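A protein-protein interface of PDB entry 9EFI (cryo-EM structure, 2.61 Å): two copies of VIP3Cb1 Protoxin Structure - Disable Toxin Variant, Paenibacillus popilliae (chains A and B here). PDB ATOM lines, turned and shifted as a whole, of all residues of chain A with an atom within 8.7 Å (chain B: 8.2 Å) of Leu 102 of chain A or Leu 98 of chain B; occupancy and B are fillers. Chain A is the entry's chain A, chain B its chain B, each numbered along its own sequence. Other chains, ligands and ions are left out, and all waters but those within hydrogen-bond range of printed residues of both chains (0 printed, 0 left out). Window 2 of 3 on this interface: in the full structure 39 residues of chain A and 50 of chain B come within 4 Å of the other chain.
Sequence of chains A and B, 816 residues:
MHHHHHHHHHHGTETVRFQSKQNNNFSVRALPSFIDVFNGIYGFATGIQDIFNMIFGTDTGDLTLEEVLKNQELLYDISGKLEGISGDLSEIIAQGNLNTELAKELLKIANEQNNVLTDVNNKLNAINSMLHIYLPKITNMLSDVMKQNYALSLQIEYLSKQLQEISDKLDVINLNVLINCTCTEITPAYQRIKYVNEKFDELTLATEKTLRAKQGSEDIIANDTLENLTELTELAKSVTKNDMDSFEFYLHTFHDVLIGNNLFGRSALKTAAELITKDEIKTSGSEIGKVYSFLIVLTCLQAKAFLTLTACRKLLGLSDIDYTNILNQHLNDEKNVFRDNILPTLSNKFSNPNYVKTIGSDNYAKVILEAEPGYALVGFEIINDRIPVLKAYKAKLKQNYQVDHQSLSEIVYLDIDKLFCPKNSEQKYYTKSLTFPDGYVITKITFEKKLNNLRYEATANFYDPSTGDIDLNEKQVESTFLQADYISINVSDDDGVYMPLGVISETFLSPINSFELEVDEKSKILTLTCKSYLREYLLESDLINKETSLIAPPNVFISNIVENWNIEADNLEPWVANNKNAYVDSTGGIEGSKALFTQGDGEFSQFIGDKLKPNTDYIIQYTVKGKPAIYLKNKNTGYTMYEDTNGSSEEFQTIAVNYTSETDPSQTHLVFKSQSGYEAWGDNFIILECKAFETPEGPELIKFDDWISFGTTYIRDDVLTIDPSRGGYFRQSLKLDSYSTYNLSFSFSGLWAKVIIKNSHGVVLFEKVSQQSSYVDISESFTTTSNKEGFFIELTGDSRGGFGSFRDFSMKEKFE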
ATOM      1  N   LEU A  89      34.304  11.415  -3.004  1.00  0.00           N
ATOM      2  CA  LEU A  89      34.166   9.990  -3.290  1.00  0.00           C
ATOM      3  C   LEU A  89      33.816   9.204  -2.032  1.00  0.00           C
ATOM      4  O   LEU A  89      32.981   8.293  -2.070  1.00  0.00           O
ATOM      5  CB  LEU A  89      35.452   9.459  -3.920  1.00  0.00           C
ATOM      6  CG  LEU A  89      35.456   7.984  -4.320  1.00  0.00           C
ATOM      7  CD1 LEU A  89      34.260   7.663  -5.198  1.00  0.00           C
ATOM      8  CD2 LEU A  89      36.748   7.642  -5.036  1.00  0.00           C
ATOM      9  N   ILE A  92      30.170   9.860  -1.102  1.00  0.00           N
ATOM     10  CA  ILE A  92      29.204   9.221  -1.995  1.00  0.00           C
ATOM     11  C   ILE A  92      29.315   7.703  -1.994  1.00  0.00           C
ATOM     12  O   ILE A  92      28.411   7.027  -2.512  1.00  0.00           O
ATOM     13  CB  ILE A  92      29.332   9.730  -3.446  1.00  0.00           C
ATOM     14  CG1 ILE A  92      30.669   9.311  -4.060  1.00  0.00           C
ATOM     15  CG2 ILE A  92      29.154  11.241  -3.502  1.00  0.00           C
ATOM     16  CD1 ILE A  92      30.558   8.189  -5.073  1.00  0.00           C
ATOM     17  N   ILE A  93      30.389   7.139  -1.437  1.00  0.00           N
ATOM     18  CA  ILE A  93      30.533   5.688  -1.396  1.00  0.00           C
ATOM     19  C   ILE A  93      29.992   5.082  -0.104  1.00  0.00           C
ATOM     20  O   ILE A  93      29.690   3.880  -0.074  1.00  0.00           O
ATOM     21  CB  ILE A  93      32.008   5.290  -1.600  1.00  0.00           C
ATOM     22  CG1 ILE A  93      32.124   3.851  -2.122  1.00  0.00           C
ATOM     23  CG2 ILE A  93      32.804   5.479  -0.314  1.00  0.00           C
ATOM     24  CD1 ILE A  93      32.493   2.818  -1.068  1.00  0.00           C
ATOM     25  N   GLY A  96      25.000   5.224  -0.327  1.00  0.00           N
ATOM     26  CA  GLY A  96      24.121   4.303  -1.012  1.00  0.00           C
ATOM     27  C   GLY A  96      24.459   2.850  -0.738  1.00  0.00           C
ATOM     28  O   GLY A  96      25.430   2.513  -0.062  1.00  0.00           O
ATOM     29  N   ASN A  97      23.613   1.969  -1.278  1.00  0.00           N
ATOM     30  CA  ASN A  97      23.853   0.535  -1.149  1.00  0.00           C
ATOM     31  C   ASN A  97      25.112   0.115  -1.900  1.00  0.00           C
ATOM     32  O   ASN A  97      25.888  -0.712  -1.407  1.00  0.00           O
ATOM     33  CB  ASN A  97      22.640  -0.245  -1.652  1.00  0.00           C
ATOM     34  CG  ASN A  97      22.801  -1.744  -1.490  1.00  0.00           C
ATOM     35  OD1 ASN A  97      23.275  -2.430  -2.394  1.00  0.00           O
ATOM     36  ND2 ASN A  97      22.407  -2.259  -0.330  1.00  0.00           N
ATOM     37  N   LEU A  98      25.319   0.662  -3.097  1.00  0.00           N
ATOM     38  CA  LEU A  98      26.490   0.423  -3.938  1.00  0.00           C
ATOM     39  C   LEU A  98      26.647  -1.035  -4.355  1.00  0.00           C
ATOM     40  O   LEU A  98      27.720  -1.417  -4.841  1.00  0.00           O
ATOM     41  CB  LEU A  98      27.780   0.906  -3.261  1.00  0.00           C
ATOM     42  CG  LEU A  98      28.158   2.372  -3.477  1.00  0.00           C
ATOM     43  CD1 LEU A  98      28.079   2.712  -4.953  1.00  0.00           C
ATOM     44  CD2 LEU A  98      27.279   3.305  -2.662  1.00  0.00           C
ATOM     45  N   ASN A  99      25.606  -1.853  -4.190  1.00  0.00           N
ATOM     46  CA  ASN A  99      25.634  -3.261  -4.579  1.00  0.00           C
ATOM     47  C   ASN A  99      26.827  -3.988  -3.970  1.00  0.00           C
ATOM     48  O   ASN A  99      27.248  -3.675  -2.852  1.00  0.00           O
ATOM     49  CB  ASN A  99      25.655  -3.395  -6.104  1.00  0.00           C
ATOM     50  CG  ASN A  99      24.510  -2.657  -6.768  1.00  0.00           C
ATOM     51  OD1 ASN A  99      23.441  -2.489  -6.181  1.00  0.00           O
ATOM     52  ND2 ASN A  99      24.730  -2.210  -7.999  1.00  0.00           N
ATOM     53  N   THR A 100      27.375  -4.961  -4.697  1.00  0.00           N
ATOM     54  CA  THR A 100      28.544  -5.705  -4.239  1.00  0.00           C
ATOM     55  C   THR A 100      29.758  -5.472  -5.129  1.00  0.00           C
ATOM     56  O   THR A 100      30.805  -5.051  -4.630  1.00  0.00           O
ATOM     57  CB  THR A 100      28.213  -7.202  -4.149  1.00  0.00           C
ATOM     58  OG1 THR A 100      29.416  -7.971  -4.262  1.00  0.00           O
ATOM     59  CG2 THR A 100      27.238  -7.605  -5.248  1.00  0.00           C
ATOM     60  N   GLU A 101      29.653  -5.728  -6.436  1.00  0.00           N
ATOM     61  CA  GLU A 101      30.786  -5.483  -7.325  1.00  0.00           C
ATOM     62  C   GLU A 101      31.054  -3.993  -7.479  1.00  0.00           C
ATOM     63  O   GLU A 101      32.215  -3.564  -7.509  1.00  0.00           O
ATOM     64  CB  GLU A 101      30.541  -6.129  -8.688  1.00  0.00           C
ATOM     65  CG  GLU A 101      31.133  -7.522  -8.834  1.00  0.00           C
ATOM     66  CD  GLU A 101      30.469  -8.541  -7.930  1.00  0.00           C
ATOM     67  OE1 GLU A 101      29.280  -8.358  -7.599  1.00  0.00           O
ATOM     68  OE2 GLU A 101      31.136  -9.527  -7.553  1.00  0.00           O
ATOM     69  N   LEU A 102      29.994  -3.187  -7.585  1.00  0.00           N
ATOM     70  CA  LEU A 102      30.170  -1.744  -7.702  1.00  0.00           C
ATOM     71  C   LEU A 102      30.831  -1.169  -6.457  1.00  0.00           C
ATOM     72  O   LEU A 102      31.699  -0.293  -6.553  1.00  0.00           O
ATOM     73  CB  LEU A 102      28.821  -1.072  -7.955  1.00  0.00           C
ATOM     74  CG  LEU A 102      28.832   0.453  -8.053  1.00  0.00           C
ATOM     75  CD1 LEU A 102      29.687   0.907  -9.225  1.00  0.00           C
ATOM     76  CD2 LEU A 102      27.416   0.986  -8.179  1.00  0.00           C
ATOM     77  N   ALA A 103      30.430  -1.649  -5.277  1.00  0.00           N
ATOM     78  CA  ALA A 103      31.052  -1.187  -4.042  1.00  0.00           C
ATOM     79  C   ALA A 103      32.531  -1.543  -4.003  1.00  0.00           C
ATOM     80  O   ALA A 103      33.362  -0.723  -3.601  1.00  0.00           O
ATOM     81  CB  ALA A 103      30.325  -1.777  -2.834  1.00  0.00           C
ATOM     82  N   LYS A 104      32.880  -2.763  -4.420  1.00  0.00           N
ATOM     83  CA  LYS A 104      34.284  -3.164  -4.444  1.00  0.00           C
ATOM     84  C   LYS A 104      35.088  -2.315  -5.421  1.00  0.00           C
ATOM     85  O   LYS A 104      36.213  -1.901  -5.115  1.00  0.00           O
ATOM     86  CB  LYS A 104      34.403  -4.647  -4.799  1.00  0.00           C
ATOM     87  CG  LYS A 104      34.526  -5.576  -3.599  1.00  0.00           C
ATOM     88  CD  LYS A 104      33.326  -5.469  -2.674  1.00  0.00           C
ATOM     89  CE  LYS A 104      33.384  -6.514  -1.572  1.00  0.00           C
ATOM     90  NZ  LYS A 104      33.374  -7.897  -2.121  1.00  0.00           N
ATOM     91  N   GLU A 105      34.530  -2.049  -6.604  1.00  0.00           N
ATOM     92  CA  GLU A 105      35.240  -1.231  -7.584  1.00  0.00           C
ATOM     93  C   GLU A 105      35.436   0.193  -7.078  1.00  0.00           C
ATOM     94  O   GLU A 105      36.519   0.772  -7.236  1.00  0.00           O
ATOM     95  CB  GLU A 105      34.489  -1.232  -8.915  1.00  0.00           C
ATOM     96  CG  GLU A 105      34.463  -2.584  -9.605  1.00  0.00           C
ATOM     97  CD  GLU A 105      35.847  -3.078  -9.977  1.00  0.00           C
ATOM     98  OE1 GLU A 105      36.726  -2.236 -10.259  1.00  0.00           O
ATOM     99  OE2 GLU A 105      36.058  -4.309  -9.986  1.00  0.00           O
ATOM    100  N   LEU A 106      34.403   0.775  -6.465  1.00  0.00           N
ATOM    101  CA  LEU A 106      34.544   2.119  -5.917  1.00  0.00           C
ATOM    102  C   LEU A 106      35.545   2.143  -4.768  1.00  0.00           C
ATOM    103  O   LEU A 106      36.300   3.109  -4.623  1.00  0.00           O
ATOM    104  CB  LEU A 106      33.189   2.657  -5.462  1.00  0.00           C
ATOM    105  CG  LEU A 106      32.249   3.122  -6.575  1.00  0.00           C
ATOM    106  CD1 LEU A 106      31.210   4.080  -6.022  1.00  0.00           C
ATOM    107  CD2 LEU A 106      33.029   3.770  -7.709  1.00  0.00           C
ATOM    108  N   LEU A 107      35.566   1.093  -3.945  1.00  0.00           N
ATOM    109  CA  LEU A 107      36.550   1.020  -2.871  1.00  0.00           C
ATOM    110  C   LEU A 107      37.965   0.948  -3.427  1.00  0.00           C
ATOM    111  O   LEU A 107      38.878   1.595  -2.905  1.00  0.00           O
ATOM    112  CB  LEU A 107      36.259  -0.185  -1.977  1.00  0.00           C
ATOM    113  CG  LEU A 107      36.245   0.065  -0.467  1.00  0.00           C
ATOM    114  CD1 LEU A 107      35.903  -1.214   0.282  1.00  0.00           C
ATOM    115  CD2 LEU A 107      37.575   0.627   0.009  1.00  0.00           C
ATOM    116  N   LYS A 108      38.168   0.167  -4.491  1.00  0.00           N
ATOM    117  CA  LYS A 108      39.492   0.085  -5.104  1.00  0.00           C
ATOM    118  C   LYS A 108      39.907   1.425  -5.703  1.00  0.00           C
ATOM    119  O   LYS A 108      41.065   1.845  -5.569  1.00  0.00           O
ATOM    120  CB  LYS A 108      39.511  -1.008  -6.170  1.00  0.00           C
ATOM    121  CG  LYS A 108      40.866  -1.203  -6.828  1.00  0.00           C
ATOM    122  CD  LYS A 108      40.805  -2.256  -7.921  1.00  0.00           C
ATOM    123  CE  LYS A 108      39.841  -1.849  -9.024  1.00  0.00           C
ATOM    124  NZ  LYS A 108      39.784  -2.865 -10.111  1.00  0.00           N
ATOM    125  N   ILE A 109      38.976   2.109  -6.372  1.00  0.00           N
ATOM    126  CA  ILE A 109      39.287   3.415  -6.950  1.00  0.00           C
ATOM    127  C   ILE A 109      39.621   4.417  -5.850  1.00  0.00           C
ATOM    128  O   ILE A 109      40.557   5.215  -5.979  1.00  0.00           O
ATOM    129  CB  ILE A 109      38.125   3.902  -7.839  1.00  0.00           C
ATOM    130  CG1 ILE A 109      38.355   3.497  -9.298  1.00  0.00           C
ATOM    131  CG2 ILE A 109      37.957   5.410  -7.745  1.00  0.00           C
ATOM    132  CD1 ILE A 109      38.379   2.006  -9.537  1.00  0.00           C
ATOM    133  N   LEU B  89      37.613   4.876 -13.539  1.00  0.00           N
ATOM    134  CA  LEU B  89      36.340   5.492 -13.181  1.00  0.00           C
ATOM    135  C   LEU B  89      35.454   5.681 -14.407  1.00  0.00           C
ATOM    136  O   LEU B  89      34.234   5.484 -14.340  1.00  0.00           O
ATOM    137  CB  LEU B  89      36.584   6.828 -12.482  1.00  0.00           C
ATOM    138  CG  LEU B  89      35.784   7.106 -11.207  1.00  0.00           C
ATOM    139  CD1 LEU B  89      36.160   8.461 -10.633  1.00  0.00           C
ATOM    140  CD2 LEU B  89      34.288   7.029 -11.467  1.00  0.00           C
ATOM    141  N   GLU B  91      35.485   3.822 -17.117  1.00  0.00           N
ATOM    142  CA  GLU B  91      34.961   2.503 -17.455  1.00  0.00           C
ATOM    143  C   GLU B  91      33.810   2.116 -16.533  1.00  0.00           C
ATOM    144  O   GLU B  91      32.788   1.589 -16.992  1.00  0.00           O
ATOM    145  CB  GLU B  91      36.073   1.457 -17.389  1.00  0.00           C
ATOM    146  CG  GLU B  91      37.124   1.598 -18.475  1.00  0.00           C
ATOM    147  CD  GLU B  91      38.173   0.508 -18.408  1.00  0.00           C
ATOM    148  OE1 GLU B  91      38.045  -0.388 -17.547  1.00  0.00           O
ATOM    149  OE2 GLU B  91      39.126   0.546 -19.214  1.00  0.00           O
ATOM    150  N   ILE B  92      33.956   2.378 -15.232  1.00  0.00           N
ATOM    151  CA  ILE B  92      32.893   2.053 -14.283  1.00  0.00           C
ATOM    152  C   ILE B  92      31.618   2.811 -14.625  1.00  0.00           C
ATOM    153  O   ILE B  92      30.518   2.245 -14.613  1.00  0.00           O
ATOM    154  CB  ILE B  92      33.355   2.343 -12.842  1.00  0.00           C
ATOM    155  CG1 ILE B  92      34.444   1.355 -12.422  1.00  0.00           C
ATOM    156  CG2 ILE B  92      32.178   2.283 -11.879  1.00  0.00           C
ATOM    157  CD1 ILE B  92      33.998  -0.089 -12.458  1.00  0.00           C
ATOM    158  N   ILE B  93      31.744   4.102 -14.937  1.00  0.00           N
ATOM    159  CA  ILE B  93      30.573   4.897 -15.296  1.00  0.00           C
ATOM    160  C   ILE B  93      29.956   4.393 -16.597  1.00  0.00           C
ATOM    161  O   ILE B  93      28.731   4.273 -16.712  1.00  0.00           O
ATOM    162  CB  ILE B  93      30.945   6.388 -15.384  1.00  0.00           C
ATOM    163  CG1 ILE B  93      31.356   6.917 -14.009  1.00  0.00           C
ATOM    164  CG2 ILE B  93      29.785   7.198 -15.941  1.00  0.00           C
ATOM    165  CD1 ILE B  93      31.727   8.383 -14.006  1.00  0.00           C
ATOM    166  N   ALA B  94      30.790   4.083 -17.592  1.00  0.00           N
ATOM    167  CA  ALA B  94      30.290   3.663 -18.895  1.00  0.00           C
ATOM    168  C   ALA B  94      29.661   2.278 -18.866  1.00  0.00           C
ATOM    169  O   ALA B  94      28.868   1.958 -19.758  1.00  0.00           O
ATOM    170  CB  ALA B  94      31.420   3.695 -19.925  1.00  0.00           C
ATOM    171  N   GLN B  95      29.994   1.450 -17.873  1.00  0.00           N
ATOM    172  CA  GLN B  95      29.372   0.134 -17.781  1.00  0.00           C
ATOM    173  C   GLN B  95      27.868   0.217 -17.550  1.00  0.00           C
ATOM    174  O   GLN B  95      27.158  -0.757 -17.822  1.00  0.00           O
ATOM    175  CB  GLN B  95      30.022  -0.687 -16.665  1.00  0.00           C
ATOM    176  CG  GLN B  95      31.400  -1.229 -17.009  1.00  0.00           C
ATOM    177  CD  GLN B  95      31.375  -2.207 -18.167  1.00  0.00           C
ATOM    178  OE1 GLN B  95      32.313  -2.269 -18.961  1.00  0.00           O
ATOM    179  NE2 GLN B  95      30.302  -2.984 -18.265  1.00  0.00           N
ATOM    180  N   GLY B  96      27.368   1.350 -17.063  1.00  0.00           N
ATOM    181  CA  GLY B  96      25.942   1.490 -16.853  1.00  0.00           C
ATOM    182  C   GLY B  96      25.456   0.689 -15.654  1.00  0.00           C
ATOM    183  O   GLY B  96      26.226   0.283 -14.779  1.00  0.00           O
ATOM    184  N   ASN B  97      24.141   0.457 -15.637  1.00  0.00           N
ATOM    185  CA  ASN B  97      23.476  -0.277 -14.559  1.00  0.00           C
ATOM    186  C   ASN B  97      23.728   0.377 -13.202  1.00  0.00           C
ATOM    187  O   ASN B  97      23.999  -0.297 -12.206  1.00  0.00           O
ATOM    188  CB  ASN B  97      23.906  -1.746 -14.542  1.00  0.00           C
ATOM    189  CG  ASN B  97      23.706  -2.427 -15.882  1.00  0.00           C
ATOM    190  OD1 ASN B  97      22.786  -2.095 -16.628  1.00  0.00           O
ATOM    191  ND2 ASN B  97      24.573  -3.384 -16.193  1.00  0.00           N
ATOM    192  N   LEU B  98      23.635   1.704 -13.162  1.00  0.00           N
ATOM    193  CA  LEU B  98      23.873   2.474 -11.952  1.00  0.00           C
ATOM    194  C   LEU B  98      22.692   3.395 -11.685  1.00  0.00           C
ATOM    195  O   LEU B  98      21.927   3.739 -12.590  1.00  0.00           O
ATOM    196  CB  LEU B  98      25.162   3.302 -12.055  1.00  0.00           C
ATOM    197  CG  LEU B  98      26.413   2.775 -11.350  1.00  0.00           C
ATOM    198  CD1 LEU B  98      26.770   1.379 -11.827  1.00  0.00           C
ATOM    199  CD2 LEU B  98      27.571   3.727 -11.574  1.00  0.00           C
ATOM    200  N   ASN B  99      22.550   3.787 -10.421  1.00  0.00           N
ATOM    201  CA  ASN B  99      21.522   4.746 -10.046  1.00  0.00           C
ATOM    202  C   ASN B  99      21.785   6.087 -10.720  1.00  0.00           C
ATOM    203  O   ASN B  99      22.937   6.487 -10.911  1.00  0.00           O
ATOM    204  CB  ASN B  99      21.482   4.915  -8.527  1.00  0.00           C
ATOM    205  CG  ASN B  99      20.375   5.845  -8.073  1.00  0.00           C
ATOM    206  OD1 ASN B  99      19.385   6.040  -8.778  1.00  0.00           O
ATOM    207  ND2 ASN B  99      20.539   6.427  -6.891  1.00  0.00           N
ATOM    208  N   THR B 100      20.706   6.780 -11.088  1.00  0.00           N
ATOM    209  CA  THR B 100      20.842   8.023 -11.841  1.00  0.00           C
ATOM    210  C   THR B 100      21.588   9.082 -11.035  1.00  0.00           C
ATOM    211  O   THR B 100      22.505   9.734 -11.547  1.00  0.00           O
ATOM    212  CB  THR B 100      19.464   8.538 -12.259  1.00  0.00           C
ATOM    213  OG1 THR B 100      18.800   7.543 -13.047  1.00  0.00           O
ATOM    214  CG2 THR B 100      19.599   9.813 -13.076  1.00  0.00           C
ATOM    215  N   GLU B 101      21.212   9.264  -9.768  1.00  0.00           N
ATOM    216  CA  GLU B 101      21.909  10.235  -8.929  1.00  0.00           C
ATOM    217  C   GLU B 101      23.340   9.795  -8.647  1.00  0.00           C
ATOM    218  O   GLU B 101      24.266  10.618  -8.658  1.00  0.00           O
ATOM    219  CB  GLU B 101      21.142  10.448  -7.624  1.00  0.00           C
ATOM    220  CG  GLU B 101      19.690  10.854  -7.819  1.00  0.00           C
ATOM    221  CD  GLU B 101      19.542  12.194  -8.514  1.00  0.00           C
ATOM    222  OE1 GLU B 101      20.440  13.049  -8.364  1.00  0.00           O
ATOM    223  OE2 GLU B 101      18.526  12.391  -9.214  1.00  0.00           O
ATOM    224  N   LEU B 102      23.537   8.501  -8.385  1.00  0.00           N
ATOM    225  CA  LEU B 102      24.884   7.984  -8.175  1.00  0.00           C
ATOM    226  C   LEU B 102      25.739   8.158  -9.423  1.00  0.00           C
ATOM    227  O   LEU B 102      26.902   8.569  -9.337  1.00  0.00           O
ATOM    228  CB  LEU B 102      24.820   6.513  -7.768  1.00  0.00           C
ATOM    229  CG  LEU B 102      26.152   5.771  -7.649  1.00  0.00           C
ATOM    230  CD1 LEU B 102      26.998   6.357  -6.533  1.00  0.00           C
ATOM    231  CD2 LEU B 102      25.912   4.288  -7.426  1.00  0.00           C
ATOM    232  N   ALA B 103      25.174   7.861 -10.594  1.00  0.00           N
ATOM    233  CA  ALA B 103      25.916   8.049 -11.835  1.00  0.00           C
ATOM    234  C   ALA B 103      26.244   9.518 -12.061  1.00  0.00           C
ATOM    235  O   ALA B 103      27.337   9.850 -12.528  1.00  0.00           O
ATOM    236  CB  ALA B 103      25.126   7.485 -13.015  1.00  0.00           C
ATOM    237  N   LYS B 104      25.312  10.414 -11.730  1.00  0.00           N
ATOM    238  CA  LYS B 104      25.553  11.839 -11.931  1.00  0.00           C
ATOM    239  C   LYS B 104      26.658  12.354 -11.014  1.00  0.00           C
ATOM    240  O   LYS B 104      27.527  13.119 -11.451  1.00  0.00           O
ATOM    241  CB  LYS B 104      24.258  12.620 -11.714  1.00  0.00           C
ATOM    242  CG  LYS B 104      24.328  14.071 -12.153  1.00  0.00           C
ATOM    243  CD  LYS B 104      22.943  14.690 -12.195  1.00  0.00           C
ATOM    244  CE  LYS B 104      22.032  13.928 -13.145  1.00  0.00           C
ATOM    245  NZ  LYS B 104      20.667  14.518 -13.199  1.00  0.00           N
ATOM    246  N   LEU B 106      29.050  10.515  -9.663  1.00  0.00           N
ATOM    247  CA  LEU B 106      30.282   9.920 -10.168  1.00  0.00           C
ATOM    248  C   LEU B 106      30.799  10.680 -11.380  1.00  0.00           C
ATOM    249  O   LEU B 106      32.007  10.891 -11.519  1.00  0.00           O
ATOM    250  CB  LEU B 106      30.056   8.448 -10.511  1.00  0.00           C
ATOM    251  CG  LEU B 106      30.024   7.479  -9.331  1.00  0.00           C
ATOM    252  CD1 LEU B 106      29.700   6.075  -9.803  1.00  0.00           C
ATOM    253  CD2 LEU B 106      31.355   7.499  -8.604  1.00  0.00           C
ATOM    254  N   LEU B 107      29.897  11.103 -12.268  1.00  0.00           N
ATOM    255  CA  LEU B 107      30.306  11.900 -13.418  1.00  0.00           C
ATOM    256  C   LEU B 107      30.895  13.234 -12.979  1.00  0.00           C
ATOM    257  O   LEU B 107      31.879  13.704 -13.559  1.00  0.00           O
ATOM    258  CB  LEU B 107      29.118  12.120 -14.354  1.00  0.00           C
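Ile 92 of chain A touches Leu 106 of chain B, but with the chains exchanged Leu 106 of chain A does not touch Ile 92 of chain B (4.5 Å).
Leu 98 of chain A touches Leu 102 of chain B, and with the chains exchanged Leu 102 of chain A touches Leu 98 of chain B.
Leu 102 of chain A touches Ile 92 of chain B, but with the chains exchanged Ile 92 of chain A does not touch Leu 102 of chain B (4.3 Å).
Leu 102 of chain B touches its own counterpart, Leu 102 of chain A.
14 positions are printed for both chains.
Among the printed residues, merely in contact across the chains: Leu 98 of chain A with Leu 102 of chain B (3.6 Å), Ile 92 of chain A with Leu 106 of chain B (3.7 Å), Leu 102 of chain A with Leu 102 of chain B (3.7 Å), Leu 102 of chain A with Leu 98 of chain B (3.7 Å), Glu 105 of chain A with Ile 92 of chain B (3.8 Å) and Leu 102 of chain A with Ile 92 of chain B (3.9 Å).
Printed residues of chain B that touch a printed residue of chain A: Ile 92, Leu 98, Leu 102 and Leu 106.
Printed residues of chain A that touch a printed residue of chain B: Ile 92, Leu 98, Leu 102 and Glu 105.
Hydrophobic or aromatic side chains of chain A that line the printed part of chain B: Ile 92, Leu 98 and Leu 102.
Among the printed residues, 6 pairs touch across the chains.
Leu 102 of chain A touches three residues of chain B.
Leu 98 of chain B touches just one residue of chain A: Leu 102 (3.7 Å).
No residue of chain B comes within 4 Å of Ala 103 of chain A.
Printed residues of chain B within 4 Å of Ile 92 of chain A: Leu 106.
Printed residues of chain A within 4 Å of Ile 92 of chain B: Leu 102 (3.9 Å) and Glu 105 (3.8 Å).
Printed residues of chain A within 4 Å of Leu 102 of chain B: Leu 98 and Leu 102.
Printed residues of chain B within 4 Å of Glu 105 of chain A: Ile 92.
Leu 107 of chain B touches none of the printed residues of chain A.
The nearest residue of chain B that does not touch Leu 102 of chain A is Leu 106 of chain B (5.2 Å).
The nearest residue of chain A that does not touch Leu 98 of chain B is Asn 99 of chain A (5.6 Å).
The backbone carbonyl oxygen of Leu 98 of chain A sits at hydrogen-bond distance from the backbone NH of Ala 103 of chain A.
The side-chain carboxylate of Glu 105 of chain A lies within salt-bridge range of the side-chain amino group of Lys 108 of chain A.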
